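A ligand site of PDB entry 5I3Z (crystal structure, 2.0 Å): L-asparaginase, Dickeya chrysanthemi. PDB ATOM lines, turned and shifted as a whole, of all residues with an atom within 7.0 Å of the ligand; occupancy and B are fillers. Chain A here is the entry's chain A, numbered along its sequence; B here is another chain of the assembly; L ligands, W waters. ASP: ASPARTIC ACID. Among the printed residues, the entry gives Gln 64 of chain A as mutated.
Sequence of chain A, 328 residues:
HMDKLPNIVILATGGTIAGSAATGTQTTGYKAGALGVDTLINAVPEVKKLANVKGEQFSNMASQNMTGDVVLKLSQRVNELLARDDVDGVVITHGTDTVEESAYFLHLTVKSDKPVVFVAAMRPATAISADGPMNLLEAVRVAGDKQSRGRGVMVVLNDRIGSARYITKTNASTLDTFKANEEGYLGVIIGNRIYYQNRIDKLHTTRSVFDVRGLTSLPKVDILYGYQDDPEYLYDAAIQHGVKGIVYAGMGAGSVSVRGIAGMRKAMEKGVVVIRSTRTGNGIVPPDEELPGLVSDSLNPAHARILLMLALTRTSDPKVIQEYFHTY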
ATOM      1  N   GLY A  14      -5.596   5.974  -6.375  1.00  0.00           N
ATOM      2  CA  GLY A  14      -4.505   5.043  -6.175  1.00  0.00           C
ATOM      3  C   GLY A  14      -3.465   5.481  -5.167  1.00  0.00           C
ATOM      4  O   GLY A  14      -3.778   6.080  -4.159  1.00  0.00           O
ATOM      5  N   GLY A  15      -2.194   5.138  -5.429  1.00  0.00           N
ATOM      6  CA  GLY A  15      -1.107   5.546  -4.546  1.00  0.00           C
ATOM      7  C   GLY A  15      -0.803   4.562  -3.432  1.00  0.00           C
ATOM      8  O   GLY A  15      -1.582   3.638  -3.160  1.00  0.00           O
ATOM      9  N   THR A  16       0.359   4.750  -2.826  1.00  0.00           N
ATOM     10  CA  THR A  16       0.774   3.972  -1.673  1.00  0.00           C
ATOM     11  C   THR A  16      -0.234   4.022  -0.502  1.00  0.00           C
ATOM     12  O   THR A  16      -0.345   3.053   0.272  1.00  0.00           O
ATOM     13  CB  THR A  16       2.156   4.452  -1.226  1.00  0.00           C
ATOM     14  OG1 THR A  16       3.096   4.190  -2.286  1.00  0.00           O
ATOM     15  CG2 THR A  16       2.629   3.779   0.063  1.00  0.00           C
ATOM     16  N   ILE A  17      -1.012   5.100  -0.413  1.00  0.00           N
ATOM     17  CA  ILE A  17      -2.124   5.146   0.562  1.00  0.00           C
ATOM     18  C   ILE A  17      -3.122   3.986   0.424  1.00  0.00           C
ATOM     19  O   ILE A  17      -3.745   3.548   1.407  1.00  0.00           O
ATOM     20  CB  ILE A  17      -2.832   6.516   0.489  1.00  0.00           C
ATOM     21  CG1 ILE A  17      -3.710   6.751   1.707  1.00  0.00           C
ATOM     22  CG2 ILE A  17      -3.569   6.696  -0.852  1.00  0.00           C
ATOM     23  CD1 ILE A  17      -4.232   8.164   1.838  1.00  0.00           C
ATOM     24  N   TYR A  30       5.105  -4.661  -3.273  1.00  0.00           N
ATOM     25  CA  TYR A  30       3.669  -4.416  -3.068  1.00  0.00           C
ATOM     26  C   TYR A  30       3.152  -3.472  -4.179  1.00  0.00           C
ATOM     27  O   TYR A  30       3.925  -2.758  -4.798  1.00  0.00           O
ATOM     28  CB  TYR A  30       3.402  -3.838  -1.653  1.00  0.00           C
ATOM     29  CG  TYR A  30       3.714  -2.367  -1.499  1.00  0.00           C
ATOM     30  CD1 TYR A  30       2.791  -1.386  -1.886  1.00  0.00           C
ATOM     31  CD2 TYR A  30       4.945  -1.935  -0.978  1.00  0.00           C
ATOM     32  CE1 TYR A  30       3.086  -0.050  -1.802  1.00  0.00           C
ATOM     33  CE2 TYR A  30       5.240  -0.590  -0.873  1.00  0.00           C
ATOM     34  CZ  TYR A  30       4.306   0.345  -1.284  1.00  0.00           C
ATOM     35  OH  TYR A  30       4.590   1.675  -1.191  1.00  0.00           O
ATOM     36  N   ALA A  32       1.016  -0.311  -5.346  1.00  0.00           N
ATOM     37  CA  ALA A  32       0.382   0.974  -5.013  1.00  0.00           C
ATOM     38  C   ALA A  32      -0.951   1.020  -5.756  1.00  0.00           C
ATOM     39  O   ALA A  32      -1.021   0.622  -6.905  1.00  0.00           O
ATOM     40  CB  ALA A  32       1.270   2.147  -5.430  1.00  0.00           C
ATOM     41  N   GLY A  33      -2.020   1.451  -5.089  1.00  0.00           N
ATOM     42  CA  GLY A  33      -3.342   1.463  -5.692  1.00  0.00           C
ATOM     43  C   GLY A  33      -3.981   0.088  -5.878  1.00  0.00           C
ATOM     44  O   GLY A  33      -4.574  -0.196  -6.921  1.00  0.00           O
ATOM     45  N   MET A  61      -4.195   3.622  -9.652  1.00  0.00           N
ATOM     46  CA  MET A  61      -2.849   3.494 -10.189  1.00  0.00           C
ATOM     47  C   MET A  61      -1.803   4.087  -9.263  1.00  0.00           C
ATOM     48  O   MET A  61      -2.076   4.994  -8.469  1.00  0.00           O
ATOM     49  CB  MET A  61      -2.790   4.207 -11.538  1.00  0.00           C
ATOM     50  CG  MET A  61      -2.907   5.728 -11.429  1.00  0.00           C
ATOM     51  SD  MET A  61      -2.840   6.510 -13.041  1.00  0.00           S
ATOM     52  CE  MET A  61      -4.559   6.326 -13.528  1.00  0.00           C
ATOM     53  N   ALA A  62      -0.575   3.653  -9.456  1.00  0.00           N
ATOM     54  CA  ALA A  62       0.608   4.329  -8.934  1.00  0.00           C
ATOM     55  C   ALA A  62       0.779   5.683  -9.617  1.00  0.00           C
ATOM     56  O   ALA A  62       0.591   5.793 -10.849  1.00  0.00           O
ATOM     57  CB  ALA A  62       1.824   3.459  -9.156  1.00  0.00           C
ATOM     58  N   SER A  63       1.043   6.750  -8.840  1.00  0.00           N
ATOM     59  CA  SER A  63       0.967   8.121  -9.398  1.00  0.00           C
ATOM     60  C   SER A  63       2.056   8.460 -10.437  1.00  0.00           C
ATOM     61  O   SER A  63       1.908   9.436 -11.184  1.00  0.00           O
ATOM     62  CB  SER A  63       0.888   9.216  -8.324  1.00  0.00           C
ATOM     63  OG  SER A  63       2.115   9.498  -7.680  1.00  0.00           O
ATOM     64  N   GLN A  64       3.140   7.681 -10.474  1.00  0.00           N
ATOM     65  CA  GLN A  64       4.140   7.852 -11.521  1.00  0.00           C
ATOM     66  C   GLN A  64       3.569   7.528 -12.902  1.00  0.00           C
ATOM     67  O   GLN A  64       4.132   7.960 -13.889  1.00  0.00           O
ATOM     68  CB  GLN A  64       5.418   7.033 -11.267  1.00  0.00           C
ATOM     69  CG  GLN A  64       5.256   5.508 -11.269  1.00  0.00           C
ATOM     70  CD  GLN A  64       4.873   4.926  -9.899  1.00  0.00           C
ATOM     71  OE1 GLN A  64       4.219   5.590  -9.076  1.00  0.00           O
ATOM     72  NE2 GLN A  64       5.352   3.717  -9.625  1.00  0.00           N
ATOM     73  N   ASN A  65       2.432   6.790 -12.948  1.00  0.00           N
ATOM     74  CA  ASN A  65       1.708   6.562 -14.179  1.00  0.00           C
ATOM     75  C   ASN A  65       0.555   7.487 -14.449  1.00  0.00           C
ATOM     76  O   ASN A  65      -0.081   7.369 -15.488  1.00  0.00           O
ATOM     77  CB  ASN A  65       1.278   5.106 -14.247  1.00  0.00           C
ATOM     78  CG  ASN A  65       2.431   4.182 -14.526  1.00  0.00           C
ATOM     79  OD1 ASN A  65       3.196   4.420 -15.447  1.00  0.00           O
ATOM     80  ND2 ASN A  65       2.598   3.150 -13.695  1.00  0.00           N
ATOM     81  N   HIS A  94      -4.321   9.841  -3.502  1.00  0.00           N
ATOM     82  CA  HIS A  94      -3.408   9.898  -4.640  1.00  0.00           C
ATOM     83  C   HIS A  94      -2.030   9.431  -4.193  1.00  0.00           C
ATOM     84  O   HIS A  94      -1.695   9.480  -3.011  1.00  0.00           O
ATOM     85  CB  HIS A  94      -3.399  11.352  -5.132  1.00  0.00           C
ATOM     86  CG  HIS A  94      -2.852  11.584  -6.509  1.00  0.00           C
ATOM     87  ND1 HIS A  94      -1.505  11.593  -6.784  1.00  0.00           N
ATOM     88  CD2 HIS A  94      -3.462  12.040  -7.628  1.00  0.00           C
ATOM     89  CE1 HIS A  94      -1.302  11.940  -8.038  1.00  0.00           C
ATOM     90  NE2 HIS A  94      -2.470  12.223  -8.576  1.00  0.00           N
ATOM     91  N   GLY A  95      -1.247   8.989  -5.144  1.00  0.00           N
ATOM     92  CA  GLY A  95       0.157   8.716  -4.862  1.00  0.00           C
ATOM     93  C   GLY A  95       0.944   9.992  -4.547  1.00  0.00           C
ATOM     94  O   GLY A  95       0.624  11.059  -5.059  1.00  0.00           O
ATOM     95  N   THR A  96       1.994   9.858  -3.738  1.00  0.00           N
ATOM     96  CA  THR A  96       2.844  10.990  -3.409  1.00  0.00           C
ATOM     97  C   THR A  96       3.717  11.500  -4.597  1.00  0.00           C
ATOM     98  O   THR A  96       4.092  12.666  -4.595  1.00  0.00           O
ATOM     99  CB  THR A  96       3.801  10.673  -2.250  1.00  0.00           C
ATOM    100  OG1 THR A  96       4.664   9.564  -2.580  1.00  0.00           O
ATOM    101  CG2 THR A  96       3.030  10.368  -0.973  1.00  0.00           C
ATOM    102  N   ASP A  97       4.109  10.615  -5.525  1.00  0.00           N
ATOM    103  CA  ASP A  97       5.177  10.920  -6.488  1.00  0.00           C
ATOM    104  C   ASP A  97       4.824  12.082  -7.437  1.00  0.00           C
ATOM    105  O   ASP A  97       5.680  12.928  -7.680  1.00  0.00           O
ATOM    106  CB  ASP A  97       5.585   9.697  -7.314  1.00  0.00           C
ATOM    107  CG  ASP A  97       6.261   8.620  -6.497  1.00  0.00           C
ATOM    108  OD1 ASP A  97       6.712   8.842  -5.365  1.00  0.00           O
ATOM    109  OD2 ASP A  97       6.338   7.492  -7.048  1.00  0.00           O
ATOM    110  N   THR A  98       3.568  12.153  -7.878  1.00  0.00           N
ATOM    111  CA  THR A  98       3.113  13.258  -8.732  1.00  0.00           C
ATOM    112  C   THR A  98       1.887  14.019  -8.226  1.00  0.00           C
ATOM    113  O   THR A  98       1.236  14.740  -8.968  1.00  0.00           O
ATOM    114  CB  THR A  98       2.854  12.765 -10.165  1.00  0.00           C
ATOM    115  OG1 THR A  98       1.682  11.935 -10.221  1.00  0.00           O
ATOM    116  CG2 THR A  98       4.051  12.034 -10.673  1.00  0.00           C
ATOM    117  N   VAL A  99       1.584  13.896  -6.924  1.00  0.00           N
ATOM    118  CA  VAL A  99       0.458  14.646  -6.348  1.00  0.00           C
ATOM    119  C   VAL A  99       0.594  16.113  -6.545  1.00  0.00           C
ATOM    120  O   VAL A  99      -0.399  16.791  -6.740  1.00  0.00           O
ATOM    121  CB  VAL A  99       0.189  14.301  -4.851  1.00  0.00           C
ATOM    122  CG1 VAL A  99       1.282  14.818  -3.946  1.00  0.00           C
ATOM    123  CG2 VAL A  99      -1.191  14.796  -4.419  1.00  0.00           C
ATOM    124  N   ALA A 120      -2.282  11.749   0.676  1.00  0.00           N
ATOM    125  CA  ALA A 120      -1.430  10.663   0.238  1.00  0.00           C
ATOM    126  C   ALA A 120      -0.737  10.041   1.430  1.00  0.00           C
ATOM    127  O   ALA A 120      -0.894  10.530   2.532  1.00  0.00           O
ATOM    128  CB  ALA A 120      -0.382  11.187  -0.757  1.00  0.00           C
ATOM    129  N   ALA A 121       0.020   8.976   1.198  1.00  0.00           N
ATOM    130  CA  ALA A 121       0.789   8.306   2.251  1.00  0.00           C
ATOM    131  C   ALA A 121       2.127   7.808   1.714  1.00  0.00           C
ATOM    132  O   ALA A 121       2.193   7.286   0.596  1.00  0.00           O
ATOM    133  CB  ALA A 121       0.003   7.130   2.808  1.00  0.00           C
ATOM    134  N   MET A 122       3.161   7.966   2.511  1.00  0.00           N
ATOM    135  CA  MET A 122       4.482   7.455   2.168  1.00  0.00           C
ATOM    136  C   MET A 122       4.661   6.006   2.526  1.00  0.00           C
ATOM    137  O   MET A 122       5.552   5.360   1.965  1.00  0.00           O
ATOM    138  CB  MET A 122       5.605   8.279   2.845  1.00  0.00           C
ATOM    139  CG  MET A 122       5.701   9.707   2.284  1.00  0.00           C
ATOM    140  SD  MET A 122       6.270   9.685   0.565  1.00  0.00           S
ATOM    141  CE  MET A 122       8.024   9.425   0.787  1.00  0.00           C
ATOM    142  N   ARG A 123       3.872   5.477   3.458  1.00  0.00           N
ATOM    143  CA  ARG A 123       3.932   4.042   3.825  1.00  0.00           C
ATOM    144  C   ARG A 123       2.631   3.370   3.419  1.00  0.00           C
ATOM    145  O   ARG A 123       1.561   3.993   3.523  1.00  0.00           O
ATOM    146  CB  ARG A 123       4.081   3.871   5.328  1.00  0.00           C
ATOM    147  CG  ARG A 123       5.433   4.287   5.890  1.00  0.00           C
ATOM    148  CD  ARG A 123       5.415   4.375   7.404  1.00  0.00           C
ATOM    149  NE  ARG A 123       6.707   4.838   7.912  1.00  0.00           N
ATOM    150  CZ  ARG A 123       6.969   5.238   9.156  1.00  0.00           C
ATOM    151  NH1 ARG A 123       6.017   5.272  10.086  1.00  0.00           N
ATOM    152  NH2 ARG A 123       8.194   5.616   9.455  1.00  0.00           N
ATOM    153  N   LYS A 169       7.160  17.471  -3.038  1.00  0.00           N
ATOM    154  CA  LYS A 169       7.809  16.338  -2.406  1.00  0.00           C
ATOM    155  C   LYS A 169       9.325  16.627  -2.403  1.00  0.00           C
ATOM    156  O   LYS A 169       9.949  16.686  -3.457  1.00  0.00           O
ATOM    157  CB  LYS A 169       7.514  15.057  -3.201  1.00  0.00           C
ATOM    158  CG  LYS A 169       7.949  13.800  -2.494  1.00  0.00           C
ATOM    159  CD  LYS A 169       7.407  12.541  -3.136  1.00  0.00           C
ATOM    160  CE  LYS A 169       7.983  11.305  -2.434  1.00  0.00           C
ATOM    161  NZ  LYS A 169       7.363  10.014  -2.886  1.00  0.00           N
ATOM    162  N   ALA A 172      12.836  11.790  -1.137  1.00  0.00           N
ATOM    163  CA  ALA A 172      12.464  10.535  -1.798  1.00  0.00           C
ATOM    164  C   ALA A 172      11.594   9.588  -0.945  1.00  0.00           C
ATOM    165  O   ALA A 172      10.656   8.993  -1.475  1.00  0.00           O
ATOM    166  CB  ALA A 172      13.703   9.791  -2.214  1.00  0.00           C
ATOM    167  N   MET B 251      10.634  10.680 -10.270  1.00  0.00           N
ATOM    168  CA  MET B 251       9.521  10.967  -9.436  1.00  0.00           C
ATOM    169  C   MET B 251       9.710  10.211  -8.117  1.00  0.00           C
ATOM    170  O   MET B 251       9.975   9.025  -8.111  1.00  0.00           O
ATOM    171  CB  MET B 251       8.205  10.507 -10.122  1.00  0.00           C
ATOM    172  CG  MET B 251       7.850  11.316 -11.351  1.00  0.00           C
ATOM    173  SD  MET B 251       6.626  10.617 -12.467  1.00  0.00           S
ATOM    174  CE  MET B 251       7.593   9.396 -13.370  1.00  0.00           C
ATOM    175  N   GLY B 252       9.593  10.906  -7.004  1.00  0.00           N
ATOM    176  CA  GLY B 252       9.718  10.287  -5.692  1.00  0.00           C
ATOM    177  C   GLY B 252      11.016   9.514  -5.528  1.00  0.00           C
ATOM    178  O   GLY B 252      12.106  10.029  -5.826  1.00  0.00           O
ATOM    179  N   ALA B 253      10.886   8.275  -5.073  1.00  0.00           N
ATOM    180  CA  ALA B 253      12.033   7.427  -4.805  1.00  0.00           C
ATOM    181  C   ALA B 253      12.495   6.666  -6.054  1.00  0.00           C
ATOM    182  O   ALA B 253      12.508   5.465  -6.090  1.00  0.00           O
ATOM    183  CB  ALA B 253      11.698   6.453  -3.669  1.00  0.00           C
ATOM    184  N   SER B 255      10.871   6.453  -8.889  1.00  0.00           N
ATOM    185  CA  SER B 255       9.755   5.717  -9.470  1.00  0.00           C
ATOM    186  C   SER B 255       9.723   6.037 -10.929  1.00  0.00           C
ATOM    187  O   SER B 255      10.009   7.177 -11.320  1.00  0.00           O
ATOM    188  CB  SER B 255       8.403   6.123  -8.879  1.00  0.00           C
ATOM    189  OG  SER B 255       8.382   5.796  -7.503  1.00  0.00           O
HETATM  190  N   ASP L   1       4.833   5.385  -6.184  1.00  0.00           N
HETATM  191  CA  ASP L   1       3.847   5.726  -5.139  1.00  0.00           C
HETATM  192  C   ASP L   1       2.857   6.659  -5.783  1.00  0.00           C
HETATM  193  O   ASP L   1       1.787   6.166  -6.094  1.00  0.00           O
HETATM  194  CB  ASP L   1       4.542   6.435  -3.961  1.00  0.00           C
HETATM  195  CG  ASP L   1       3.582   6.892  -2.887  1.00  0.00           C
HETATM  196  OD1 ASP L   1       2.363   7.056  -3.175  1.00  0.00           O
HETATM  197  OD2 ASP L   1       4.064   7.108  -1.734  1.00  0.00           O
HETATM  198  OXT ASP L   1       3.140   7.871  -6.040  1.00  0.00           O
HETATM  199  O   HOH W   1       4.452   2.302  -7.074  1.00  0.00           O
HETATM  200  O   HOH W   2       6.136   6.212  -0.593  1.00  0.00           O
HETATM  201  O   HOH W   3      -0.152   7.674  -1.556  1.00  0.00           O
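N of Ser 63 is in hydrogen-bond range of O of the ligand (2.9 Å). An oxygen (OXT) of the ligand lies within hydrogen-bond range of the side-chain hydroxyl (OG) of Ser 63 (2.5 Å). N of Thr 96 lies within hydrogen-bond range of OD1 of the ligand, at 2.9 Å. OD2 of the ligand sits at hydrogen-bond distance from OG1 of Thr 96, 2.7 Å away. N of Asp 97 lies within hydrogen-bond range of OXT of the ligand. A nitrogen (N) of the ligand lies within salt-bridge range of the side-chain carboxylate of Asp 97 (2.7 Å). N of Thr 16 is in hydrogen-bond range of OD1 of the ligand, at 3.1 Å. The side-chain hydroxyl (OG1) of Thr 16 lies close to an oxygen (OD1) of the ligand (3.1 Å). The side-chain amide oxygen of Gln 64 lies within hydrogen-bond range of a nitrogen (N) of the ligand (3.0 Å). The backbone carbonyl oxygen of Ala 121 sits close to an oxygen (OD2) of the ligand, 3.0 Å away.
Water W2 bridges an oxygen (OD2) of the ligand (2.5 Å) and the backbone carbonyl oxygen of Met 122 (2.8 Å). Water W1 lies within hydrogen-bond range of NE2 of Gln 64 (3.1 Å) and N of the ligand (3.2 Å).
N of Asp 97 is in hydrogen-bond range of OG of Ser 63 (3.1 Å). The side-chain hydroxyl (OG) of Ser 63 lies close to the backbone carbonyl oxygen (O) of Gly 95, at 3.4 Å. O of Ser 63 is in hydrogen-bond range of OG1 of Thr 98 (2.7 Å). The side-chain hydroxyl of Thr 96 sits at hydrogen-bond distance from the side-chain sulfur of Met 122 (3.5 Å). The side-chain hydroxyl (OG1) of Thr 96 is in hydrogen-bond range of the side-chain amino group (NZ) of Lys 169, at 2.8 Å. OD2 of Asp 97 sits close to OE1 of Gln 64 (3.5 Å). The side-chain carboxylate (OD2) of Asp 97 sits at hydrogen-bond distance from the side-chain hydroxyl (OG) of Ser 255 of chain B, 2.7 Å away. The backbone carbonyl oxygen (O) of Gly 15 sits at hydrogen-bond distance from the backbone NH (N) of Gly 33 (2.9 Å).
Residues that only touch the ligand: Gly 95 (3.2 Å), Gly 15 (3.3 Å), Ala 62 (3.6 Å), Ser 255 of chain B (3.8 Å) and Met 122 (3.9 Å). Of the 28 residues printed, 11 come within 4 Å of the ligand. The nearest printed residue that does not touch the ligand is Ala 32 (4.1 Å).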
